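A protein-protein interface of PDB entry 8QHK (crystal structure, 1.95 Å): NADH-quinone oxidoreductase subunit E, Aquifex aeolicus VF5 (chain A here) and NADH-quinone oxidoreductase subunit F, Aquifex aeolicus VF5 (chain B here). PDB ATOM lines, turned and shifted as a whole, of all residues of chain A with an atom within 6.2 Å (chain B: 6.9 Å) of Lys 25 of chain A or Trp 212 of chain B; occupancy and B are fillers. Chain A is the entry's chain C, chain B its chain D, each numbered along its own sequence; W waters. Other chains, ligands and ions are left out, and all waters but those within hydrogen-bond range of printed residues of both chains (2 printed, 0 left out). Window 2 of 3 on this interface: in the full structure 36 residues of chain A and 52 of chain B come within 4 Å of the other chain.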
ATOM      1  N   ILE A  20     -25.351  -9.565 -19.743  1.00  0.00           N
ATOM      2  CA  ILE A  20     -24.241  -9.027 -20.518  1.00  0.00           C
ATOM      3  C   ILE A  20     -23.461  -8.010 -19.684  1.00  0.00           C
ATOM      4  O   ILE A  20     -22.255  -7.849 -19.873  1.00  0.00           O
ATOM      5  CB  ILE A  20     -24.762  -8.436 -21.846  1.00  0.00           C
ATOM      6  CG1 ILE A  20     -25.296  -9.545 -22.755  1.00  0.00           C
ATOM      7  CG2 ILE A  20     -23.700  -7.597 -22.548  1.00  0.00           C
ATOM      8  CD1 ILE A  20     -26.080  -9.050 -23.940  1.00  0.00           C
ATOM      9  N   PHE A  23     -20.753  -9.931 -16.104  1.00  0.00           N
ATOM     10  CA  PHE A  23     -19.344 -10.287 -16.132  1.00  0.00           C
ATOM     11  C   PHE A  23     -18.504  -9.095 -16.592  1.00  0.00           C
ATOM     12  O   PHE A  23     -19.025  -8.157 -17.204  1.00  0.00           O
ATOM     13  CB  PHE A  23     -19.121 -11.484 -17.056  1.00  0.00           C
ATOM     14  CG  PHE A  23     -19.812 -12.751 -16.630  1.00  0.00           C
ATOM     15  CD1 PHE A  23     -19.272 -13.553 -15.637  1.00  0.00           C
ATOM     16  CD2 PHE A  23     -20.994 -13.155 -17.231  1.00  0.00           C
ATOM     17  CE1 PHE A  23     -19.894 -14.732 -15.257  1.00  0.00           C
ATOM     18  CE2 PHE A  23     -21.625 -14.323 -16.837  1.00  0.00           C
ATOM     19  CZ  PHE A  23     -21.070 -15.116 -15.860  1.00  0.00           C
ATOM     20  N   PRO A  24     -17.177  -9.082 -16.320  1.00  0.00           N
ATOM     21  CA  PRO A  24     -16.304  -8.029 -16.841  1.00  0.00           C
ATOM     22  C   PRO A  24     -16.341  -7.838 -18.359  1.00  0.00           C
ATOM     23  O   PRO A  24     -16.241  -6.709 -18.817  1.00  0.00           O
ATOM     24  CB  PRO A  24     -14.906  -8.474 -16.396  1.00  0.00           C
ATOM     25  CG  PRO A  24     -15.170  -9.275 -15.140  1.00  0.00           C
ATOM     26  CD  PRO A  24     -16.458 -10.016 -15.435  1.00  0.00           C
ATOM     27  N   LYS A  25     -16.464  -8.937 -19.121  1.00  0.00           N
ATOM     28  CA  LYS A  25     -16.501  -8.885 -20.576  1.00  0.00           C
ATOM     29  C   LYS A  25     -17.826  -9.466 -21.060  1.00  0.00           C
ATOM     30  O   LYS A  25     -18.296 -10.469 -20.528  1.00  0.00           O
ATOM     31  CB  LYS A  25     -15.313  -9.646 -21.176  1.00  0.00           C
ATOM     32  CG  LYS A  25     -13.944  -9.204 -20.681  1.00  0.00           C
ATOM     33  CD  LYS A  25     -12.798  -9.770 -21.490  1.00  0.00           C
ATOM     34  CE  LYS A  25     -11.445  -9.452 -20.885  1.00  0.00           C
ATOM     35  NZ  LYS A  25     -10.331  -9.972 -21.715  1.00  0.00           N
ATOM     36  N   LYS A  26     -18.415  -8.822 -22.076  1.00  0.00           N
ATOM     37  CA  LYS A  26     -19.761  -9.137 -22.537  1.00  0.00           C
ATOM     38  C   LYS A  26     -19.880 -10.595 -22.971  1.00  0.00           C
ATOM     39  O   LYS A  26     -20.897 -11.232 -22.706  1.00  0.00           O
ATOM     40  CB  LYS A  26     -20.171  -8.260 -23.725  1.00  0.00           C
ATOM     41  CG  LYS A  26     -20.349  -6.779 -23.423  1.00  0.00           C
ATOM     42  CD  LYS A  26     -20.797  -5.970 -24.630  1.00  0.00           C
ATOM     43  CE  LYS A  26     -21.185  -4.547 -24.285  1.00  0.00           C
ATOM     44  NZ  LYS A  26     -20.109  -3.859 -23.528  1.00  0.00           N
ATOM     45  N   ARG A  27     -18.841 -11.113 -23.638  1.00  0.00           N
ATOM     46  CA  ARG A  27     -18.926 -12.413 -24.288  1.00  0.00           C
ATOM     47  C   ARG A  27     -19.024 -13.547 -23.270  1.00  0.00           C
ATOM     48  O   ARG A  27     -19.468 -14.634 -23.629  1.00  0.00           O
ATOM     49  CB  ARG A  27     -17.770 -12.630 -25.271  1.00  0.00           C
ATOM     50  CG  ARG A  27     -16.375 -12.673 -24.662  1.00  0.00           C
ATOM     51  CD  ARG A  27     -15.375 -12.472 -25.783  1.00  0.00           C
ATOM     52  NE  ARG A  27     -14.000 -12.329 -25.339  1.00  0.00           N
ATOM     53  CZ  ARG A  27     -13.368 -11.170 -25.206  1.00  0.00           C
ATOM     54  NH1 ARG A  27     -12.064 -11.151 -24.997  1.00  0.00           N
ATOM     55  NH2 ARG A  27     -14.037 -10.033 -25.316  1.00  0.00           N
ATOM     56  N   GLN A  28     -18.679 -13.286 -22.000  1.00  0.00           N
ATOM     57  CA  GLN A  28     -18.789 -14.304 -20.962  1.00  0.00           C
ATOM     58  C   GLN A  28     -20.252 -14.630 -20.659  1.00  0.00           C
ATOM     59  O   GLN A  28     -20.541 -15.670 -20.083  1.00  0.00           O
ATOM     60  CB  GLN A  28     -18.077 -13.863 -19.681  1.00  0.00           C
ATOM     61  CG  GLN A  28     -16.640 -13.433 -19.917  1.00  0.00           C
ATOM     62  CD  GLN A  28     -15.927 -13.134 -18.627  1.00  0.00           C
ATOM     63  OE1 GLN A  28     -15.729 -11.976 -18.269  1.00  0.00           O
ATOM     64  NE2 GLN A  28     -15.536 -14.187 -17.930  1.00  0.00           N
ATOM     65  N   ALA A  29     -21.178 -13.744 -21.049  1.00  0.00           N
ATOM     66  CA  ALA A  29     -22.586 -13.914 -20.726  1.00  0.00           C
ATOM     67  C   ALA A  29     -23.315 -14.835 -21.708  1.00  0.00           C
ATOM     68  O   ALA A  29     -24.536 -14.958 -21.610  1.00  0.00           O
ATOM     69  CB  ALA A  29     -23.244 -12.553 -20.711  1.00  0.00           C
ATOM     70  N   TYR B  88      -6.478 -14.990 -11.258  1.00  0.00           N
ATOM     71  CA  TYR B  88      -7.871 -15.361 -11.137  1.00  0.00           C
ATOM     72  C   TYR B  88      -8.007 -16.653 -10.340  1.00  0.00           C
ATOM     73  O   TYR B  88      -7.171 -17.544 -10.430  1.00  0.00           O
ATOM     74  CB  TYR B  88      -8.504 -15.535 -12.522  1.00  0.00           C
ATOM     75  CG  TYR B  88      -8.444 -14.304 -13.383  1.00  0.00           C
ATOM     76  CD1 TYR B  88      -9.102 -13.147 -13.004  1.00  0.00           C
ATOM     77  CD2 TYR B  88      -7.719 -14.286 -14.564  1.00  0.00           C
ATOM     78  CE1 TYR B  88      -9.059 -12.006 -13.784  1.00  0.00           C
ATOM     79  CE2 TYR B  88      -7.652 -13.148 -15.348  1.00  0.00           C
ATOM     80  CZ  TYR B  88      -8.326 -12.003 -14.959  1.00  0.00           C
ATOM     81  OH  TYR B  88      -8.289 -10.861 -15.726  1.00  0.00           O
ATOM     82  N   GLU B 129     -10.755 -11.213  -8.590  1.00  0.00           N
ATOM     83  CA  GLU B 129     -11.855 -11.664  -9.414  1.00  0.00           C
ATOM     84  C   GLU B 129     -11.881 -13.186  -9.333  1.00  0.00           C
ATOM     85  O   GLU B 129     -10.879 -13.846  -9.613  1.00  0.00           O
ATOM     86  CB  GLU B 129     -11.652 -11.087 -10.813  1.00  0.00           C
ATOM     87  CG  GLU B 129     -12.664 -11.534 -11.842  1.00  0.00           C
ATOM     88  CD  GLU B 129     -12.478 -10.871 -13.204  1.00  0.00           C
ATOM     89  OE1 GLU B 129     -12.271  -9.635 -13.241  1.00  0.00           O
ATOM     90  OE2 GLU B 129     -12.564 -11.587 -14.229  1.00  0.00           O
ATOM     91  N   TYR B 131     -14.488 -16.867  -9.833  1.00  0.00           N
ATOM     92  CA  TYR B 131     -15.643 -17.409 -10.525  1.00  0.00           C
ATOM     93  C   TYR B 131     -16.061 -18.722  -9.886  1.00  0.00           C
ATOM     94  O   TYR B 131     -15.216 -19.470  -9.396  1.00  0.00           O
ATOM     95  CB  TYR B 131     -15.332 -17.675 -11.996  1.00  0.00           C
ATOM     96  CG  TYR B 131     -15.031 -16.437 -12.785  1.00  0.00           C
ATOM     97  CD1 TYR B 131     -13.781 -15.850 -12.736  1.00  0.00           C
ATOM     98  CD2 TYR B 131     -16.020 -15.834 -13.544  1.00  0.00           C
ATOM     99  CE1 TYR B 131     -13.507 -14.699 -13.449  1.00  0.00           C
ATOM    100  CE2 TYR B 131     -15.762 -14.690 -14.270  1.00  0.00           C
ATOM    101  CZ  TYR B 131     -14.501 -14.129 -14.226  1.00  0.00           C
ATOM    102  OH  TYR B 131     -14.254 -12.996 -14.937  1.00  0.00           O
ATOM    103  N   ILE B 189     -12.223 -22.983 -18.452  1.00  0.00           N
ATOM    104  CA  ILE B 189     -11.724 -21.645 -18.725  1.00  0.00           C
ATOM    105  C   ILE B 189     -12.182 -21.187 -20.111  1.00  0.00           C
ATOM    106  O   ILE B 189     -12.655 -20.059 -20.253  1.00  0.00           O
ATOM    107  CB  ILE B 189     -10.197 -21.596 -18.540  1.00  0.00           C
ATOM    108  CG1 ILE B 189      -9.822 -21.748 -17.063  1.00  0.00           C
ATOM    109  CG2 ILE B 189      -9.622 -20.334 -19.158  1.00  0.00           C
ATOM    110  CD1 ILE B 189      -8.360 -22.043 -16.797  1.00  0.00           C
ATOM    111  N   LEU B 192     -15.712 -20.171 -19.780  1.00  0.00           N
ATOM    112  CA  LEU B 192     -15.778 -18.896 -19.074  1.00  0.00           C
ATOM    113  C   LEU B 192     -15.447 -17.734 -20.003  1.00  0.00           C
ATOM    114  O   LEU B 192     -15.912 -16.623 -19.768  1.00  0.00           O
ATOM    115  CB  LEU B 192     -14.778 -18.876 -17.916  1.00  0.00           C
ATOM    116  CG  LEU B 192     -15.283 -19.345 -16.564  1.00  0.00           C
ATOM    117  CD1 LEU B 192     -14.178 -19.186 -15.531  1.00  0.00           C
ATOM    118  CD2 LEU B 192     -16.522 -18.570 -16.145  1.00  0.00           C
ATOM    119  N   GLU B 193     -14.591 -17.986 -21.004  1.00  0.00           N
ATOM    120  CA  GLU B 193     -14.213 -16.976 -21.975  1.00  0.00           C
ATOM    121  C   GLU B 193     -15.252 -16.899 -23.100  1.00  0.00           C
ATOM    122  O   GLU B 193     -15.018 -16.227 -24.106  1.00  0.00           O
ATOM    123  CB  GLU B 193     -12.813 -17.274 -22.519  1.00  0.00           C
ATOM    124  CG  GLU B 193     -11.700 -17.110 -21.504  1.00  0.00           C
ATOM    125  CD  GLU B 193     -10.316 -17.503 -22.004  1.00  0.00           C
ATOM    126  OE1 GLU B 193      -9.334 -17.302 -21.267  1.00  0.00           O
ATOM    127  OE2 GLU B 193     -10.218 -18.035 -23.130  1.00  0.00           O
ATOM    128  N   GLY B 194     -16.382 -17.604 -22.951  1.00  0.00           N
ATOM    129  CA  GLY B 194     -17.515 -17.456 -23.856  1.00  0.00           C
ATOM    130  C   GLY B 194     -17.407 -18.323 -25.110  1.00  0.00           C
ATOM    131  O   GLY B 194     -18.070 -18.056 -26.106  1.00  0.00           O
ATOM    132  N   LYS B 195     -16.609 -19.388 -25.030  1.00  0.00           N
ATOM    133  CA  LYS B 195     -16.350 -20.260 -26.163  1.00  0.00           C
ATOM    134  C   LYS B 195     -16.826 -21.678 -25.867  1.00  0.00           C
ATOM    135  O   LYS B 195     -17.272 -21.985 -24.757  1.00  0.00           O
ATOM    136  CB  LYS B 195     -14.853 -20.270 -26.479  1.00  0.00           C
ATOM    137  CG  LYS B 195     -14.324 -18.994 -27.115  1.00  0.00           C
ATOM    138  CD  LYS B 195     -12.810 -18.946 -27.189  1.00  0.00           C
ATOM    139  CE  LYS B 195     -12.180 -18.810 -25.819  1.00  0.00           C
ATOM    140  NZ  LYS B 195     -10.712 -18.631 -25.904  1.00  0.00           N
ATOM    141  N   ARG B 200      -7.353 -27.353 -23.609  1.00  0.00           N
ATOM    142  CA  ARG B 200      -6.114 -26.849 -24.173  1.00  0.00           C
ATOM    143  C   ARG B 200      -4.995 -27.824 -23.817  1.00  0.00           C
ATOM    144  O   ARG B 200      -5.045 -28.476 -22.777  1.00  0.00           O
ATOM    145  CB  ARG B 200      -5.716 -25.489 -23.585  1.00  0.00           C
ATOM    146  CG  ARG B 200      -6.765 -24.384 -23.625  1.00  0.00           C
ATOM    147  CD  ARG B 200      -6.312 -23.229 -22.725  1.00  0.00           C
ATOM    148  NE  ARG B 200      -7.157 -22.036 -22.728  1.00  0.00           N
ATOM    149  CZ  ARG B 200      -6.967 -20.965 -21.949  1.00  0.00           C
ATOM    150  NH1 ARG B 200      -6.009 -20.948 -21.034  1.00  0.00           N
ATOM    151  NH2 ARG B 200      -7.756 -19.913 -22.081  1.00  0.00           N
ATOM    152  N   LYS B 209      -0.757 -20.112 -17.184  1.00  0.00           N
ATOM    153  CA  LYS B 209      -1.540 -19.431 -18.201  1.00  0.00           C
ATOM    154  C   LYS B 209      -2.950 -20.015 -18.190  1.00  0.00           C
ATOM    155  O   LYS B 209      -3.130 -21.181 -18.514  1.00  0.00           O
ATOM    156  CB  LYS B 209      -0.833 -19.575 -19.556  1.00  0.00           C
ATOM    157  CG  LYS B 209      -1.519 -18.904 -20.737  1.00  0.00           C
ATOM    158  N   GLY B 210      -3.933 -19.194 -17.793  1.00  0.00           N
ATOM    159  CA  GLY B 210      -5.312 -19.631 -17.656  1.00  0.00           C
ATOM    160  C   GLY B 210      -6.308 -18.651 -18.281  1.00  0.00           C
ATOM    161  O   GLY B 210      -6.282 -18.403 -19.487  1.00  0.00           O
ATOM    162  N   LEU B 211      -7.210 -18.123 -17.451  1.00  0.00           N
ATOM    163  CA  LEU B 211      -8.241 -17.200 -17.910  1.00  0.00           C
ATOM    164  C   LEU B 211      -7.585 -15.927 -18.440  1.00  0.00           C
ATOM    165  O   LEU B 211      -6.787 -15.312 -17.735  1.00  0.00           O
ATOM    166  CB  LEU B 211      -9.187 -16.901 -16.743  1.00  0.00           C
ATOM    167  CG  LEU B 211     -10.366 -15.976 -17.062  1.00  0.00           C
ATOM    168  CD1 LEU B 211     -11.340 -16.648 -18.024  1.00  0.00           C
ATOM    169  CD2 LEU B 211     -11.090 -15.551 -15.787  1.00  0.00           C
ATOM    170  N   TRP B 212      -7.912 -15.578 -19.698  1.00  0.00           N
ATOM    171  CA  TRP B 212      -7.310 -14.471 -20.435  1.00  0.00           C
ATOM    172  C   TRP B 212      -5.785 -14.581 -20.455  1.00  0.00           C
ATOM    173  O   TRP B 212      -5.095 -13.567 -20.525  1.00  0.00           O
ATOM    174  CB  TRP B 212      -7.759 -13.115 -19.864  1.00  0.00           C
ATOM    175  CG  TRP B 212      -9.239 -13.005 -19.665  1.00  0.00           C
ATOM    176  CD1 TRP B 212      -9.885 -12.678 -18.510  1.00  0.00           C
ATOM    177  CD2 TRP B 212     -10.269 -13.271 -20.636  1.00  0.00           C
ATOM    178  NE1 TRP B 212     -11.238 -12.702 -18.694  1.00  0.00           N
ATOM    179  CE2 TRP B 212     -11.507 -13.065 -19.985  1.00  0.00           C
ATOM    180  CE3 TRP B 212     -10.270 -13.662 -21.981  1.00  0.00           C
ATOM    181  CZ2 TRP B 212     -12.728 -13.235 -20.634  1.00  0.00           C
ATOM    182  CZ3 TRP B 212     -11.478 -13.817 -22.624  1.00  0.00           C
ATOM    183  CH2 TRP B 212     -12.688 -13.615 -21.957  1.00  0.00           C
ATOM    184  N   GLY B 213      -5.264 -15.810 -20.367  1.00  0.00           N
ATOM    185  CA  GLY B 213      -3.829 -16.040 -20.385  1.00  0.00           C
ATOM    186  C   GLY B 213      -3.132 -15.753 -19.055  1.00  0.00           C
ATOM    187  O   GLY B 213      -1.921 -15.885 -18.979  1.00  0.00           O
ATOM    188  N   LYS B 214      -3.885 -15.418 -17.998  1.00  0.00           N
ATOM    189  CA  LYS B 214      -3.297 -14.969 -16.743  1.00  0.00           C
ATOM    190  C   LYS B 214      -3.189 -16.125 -15.757  1.00  0.00           C
ATOM    191  O   LYS B 214      -3.932 -17.093 -15.857  1.00  0.00           O
ATOM    192  CB  LYS B 214      -4.151 -13.872 -16.108  1.00  0.00           C
ATOM    193  CG  LYS B 214      -4.357 -12.635 -16.966  1.00  0.00           C
ATOM    194  CD  LYS B 214      -3.073 -12.088 -17.536  1.00  0.00           C
ATOM    195  CE  LYS B 214      -3.185 -10.633 -17.933  1.00  0.00           C
ATOM    196  NZ  LYS B 214      -1.894 -10.108 -18.431  1.00  0.00           N
ATOM    197  N   PRO B 215      -2.276 -16.058 -14.756  1.00  0.00           N
ATOM    198  CA  PRO B 215      -2.216 -17.078 -13.709  1.00  0.00           C
ATOM    199  C   PRO B 215      -3.591 -17.289 -13.086  1.00  0.00           C
ATOM    200  O   PRO B 215      -4.241 -16.331 -12.661  1.00  0.00           O
ATOM    201  CB  PRO B 215      -1.195 -16.509 -12.715  1.00  0.00           C
ATOM    202  CG  PRO B 215      -0.297 -15.670 -13.593  1.00  0.00           C
ATOM    203  CD  PRO B 215      -1.248 -15.024 -14.582  1.00  0.00           C
ATOM    204  N   THR B 216      -4.007 -18.558 -13.052  1.00  0.00           N
ATOM    205  CA  THR B 216      -5.339 -18.944 -12.639  1.00  0.00           C
ATOM    206  C   THR B 216      -5.267 -20.230 -11.823  1.00  0.00           C
ATOM    207  O   THR B 216      -4.727 -21.227 -12.290  1.00  0.00           O
ATOM    208  CB  THR B 216      -6.227 -19.170 -13.870  1.00  0.00           C
ATOM    209  OG1 THR B 216      -6.207 -17.984 -14.667  1.00  0.00           O
ATOM    210  CG2 THR B 216      -7.640 -19.562 -13.510  1.00  0.00           C
HETATM  211  O   HOH W   1     -13.156 -14.991 -25.693  1.00  0.00           O
HETATM  212  O   HOH W   2     -13.191 -11.389 -16.962  1.00  0.00           O
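Water W1 bridges the backbone carbonyl oxygen (O) of Glu 193 of chain B (2.7 Å) and the guanidinium group (NE) of Arg 27 of chain A (2.8 Å).
Water W2 lies within hydrogen-bond range of the side-chain hydroxyl of Tyr 131 of chain B (2.8 Å), the side-chain carboxylate of Glu 129 of chain B (2.8 Å), the side-chain amide oxygen of Gln 28 of chain A (2.9 Å) and the indole nitrogen of Trp 212 of chain B (2.9 Å).
Of the 8 printed residues of chain A, 5 touch a printed residue of chain B.
Among the printed residues, pairs that only touch across the chains: Phe 23 of chain A with Tyr 131 of chain B, Pro 24 of chain A with Glu 129 of chain B, Pro 24 of chain A with Tyr 131 of chain B, Lys 25 of chain A with Trp 212 of chain B, Arg 27 of chain A with Glu 193 of chain B, Arg 27 of chain A with Gly 194 of chain B, Arg 27 of chain A with Trp 212 of chain B and Gln 28 of chain A with Trp 212 of chain B.
O of Leu 192 of chain B is in hydrogen-bond range of NE2 of Gln 28 of chain A (3.1 Å).
The side-chain amide nitrogen (NE2) of Gln 28 of chain A sits at hydrogen-bond distance from the side-chain hydroxyl (OH) of Tyr 131 of chain B, at 3.5 Å.
The side-chain carboxylate of Glu 193 of chain B is in salt-bridge range of the side-chain amino group of Lys 195 of chain B.
The backbone NH of Lys 25 of chain A is in hydrogen-bond range of the side-chain amide oxygen of Gln 28 of chain A (3.2 Å).
The side-chain carboxylate (OE1) of Glu 193 of chain B sits at hydrogen-bond distance from the backbone NH (N) of Trp 212 of chain B (2.7 Å).
The guanidinium group of Arg 200 of chain B is in salt-bridge range of the side-chain carboxylate of Glu 193 of chain B (3.2 Å).
Of the printed residues of chain B, Phe 23 of chain A touches Tyr 131 (3.9 Å).
Printed residues of chain B within 4 Å of Pro 24 of chain A: Glu 129 (3.5 Å) and Tyr 131 (3.7 Å).
Lys 25 of chain A touches just one residue of chain B: Trp 212.
Printed residues of chain A within 4 Å of Tyr 131 of chain B: Phe 23, Pro 24 and Gln 28.
Printed residues of chain A within 4 Å of Glu 193 of chain B: Arg 27 (3.8 Å).
Gly 210 of chain B touches none of the printed residues of chain A.
Trp 212 of chain B touches just these residues of chain A: Lys 25 (3.5 Å), Arg 27 (3.6 Å) and Gln 28 (3.8 Å).
The nearest printed residue of chain A that does not touch Gly 194 of chain B is Gln 28 of chain A (4.5 Å).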
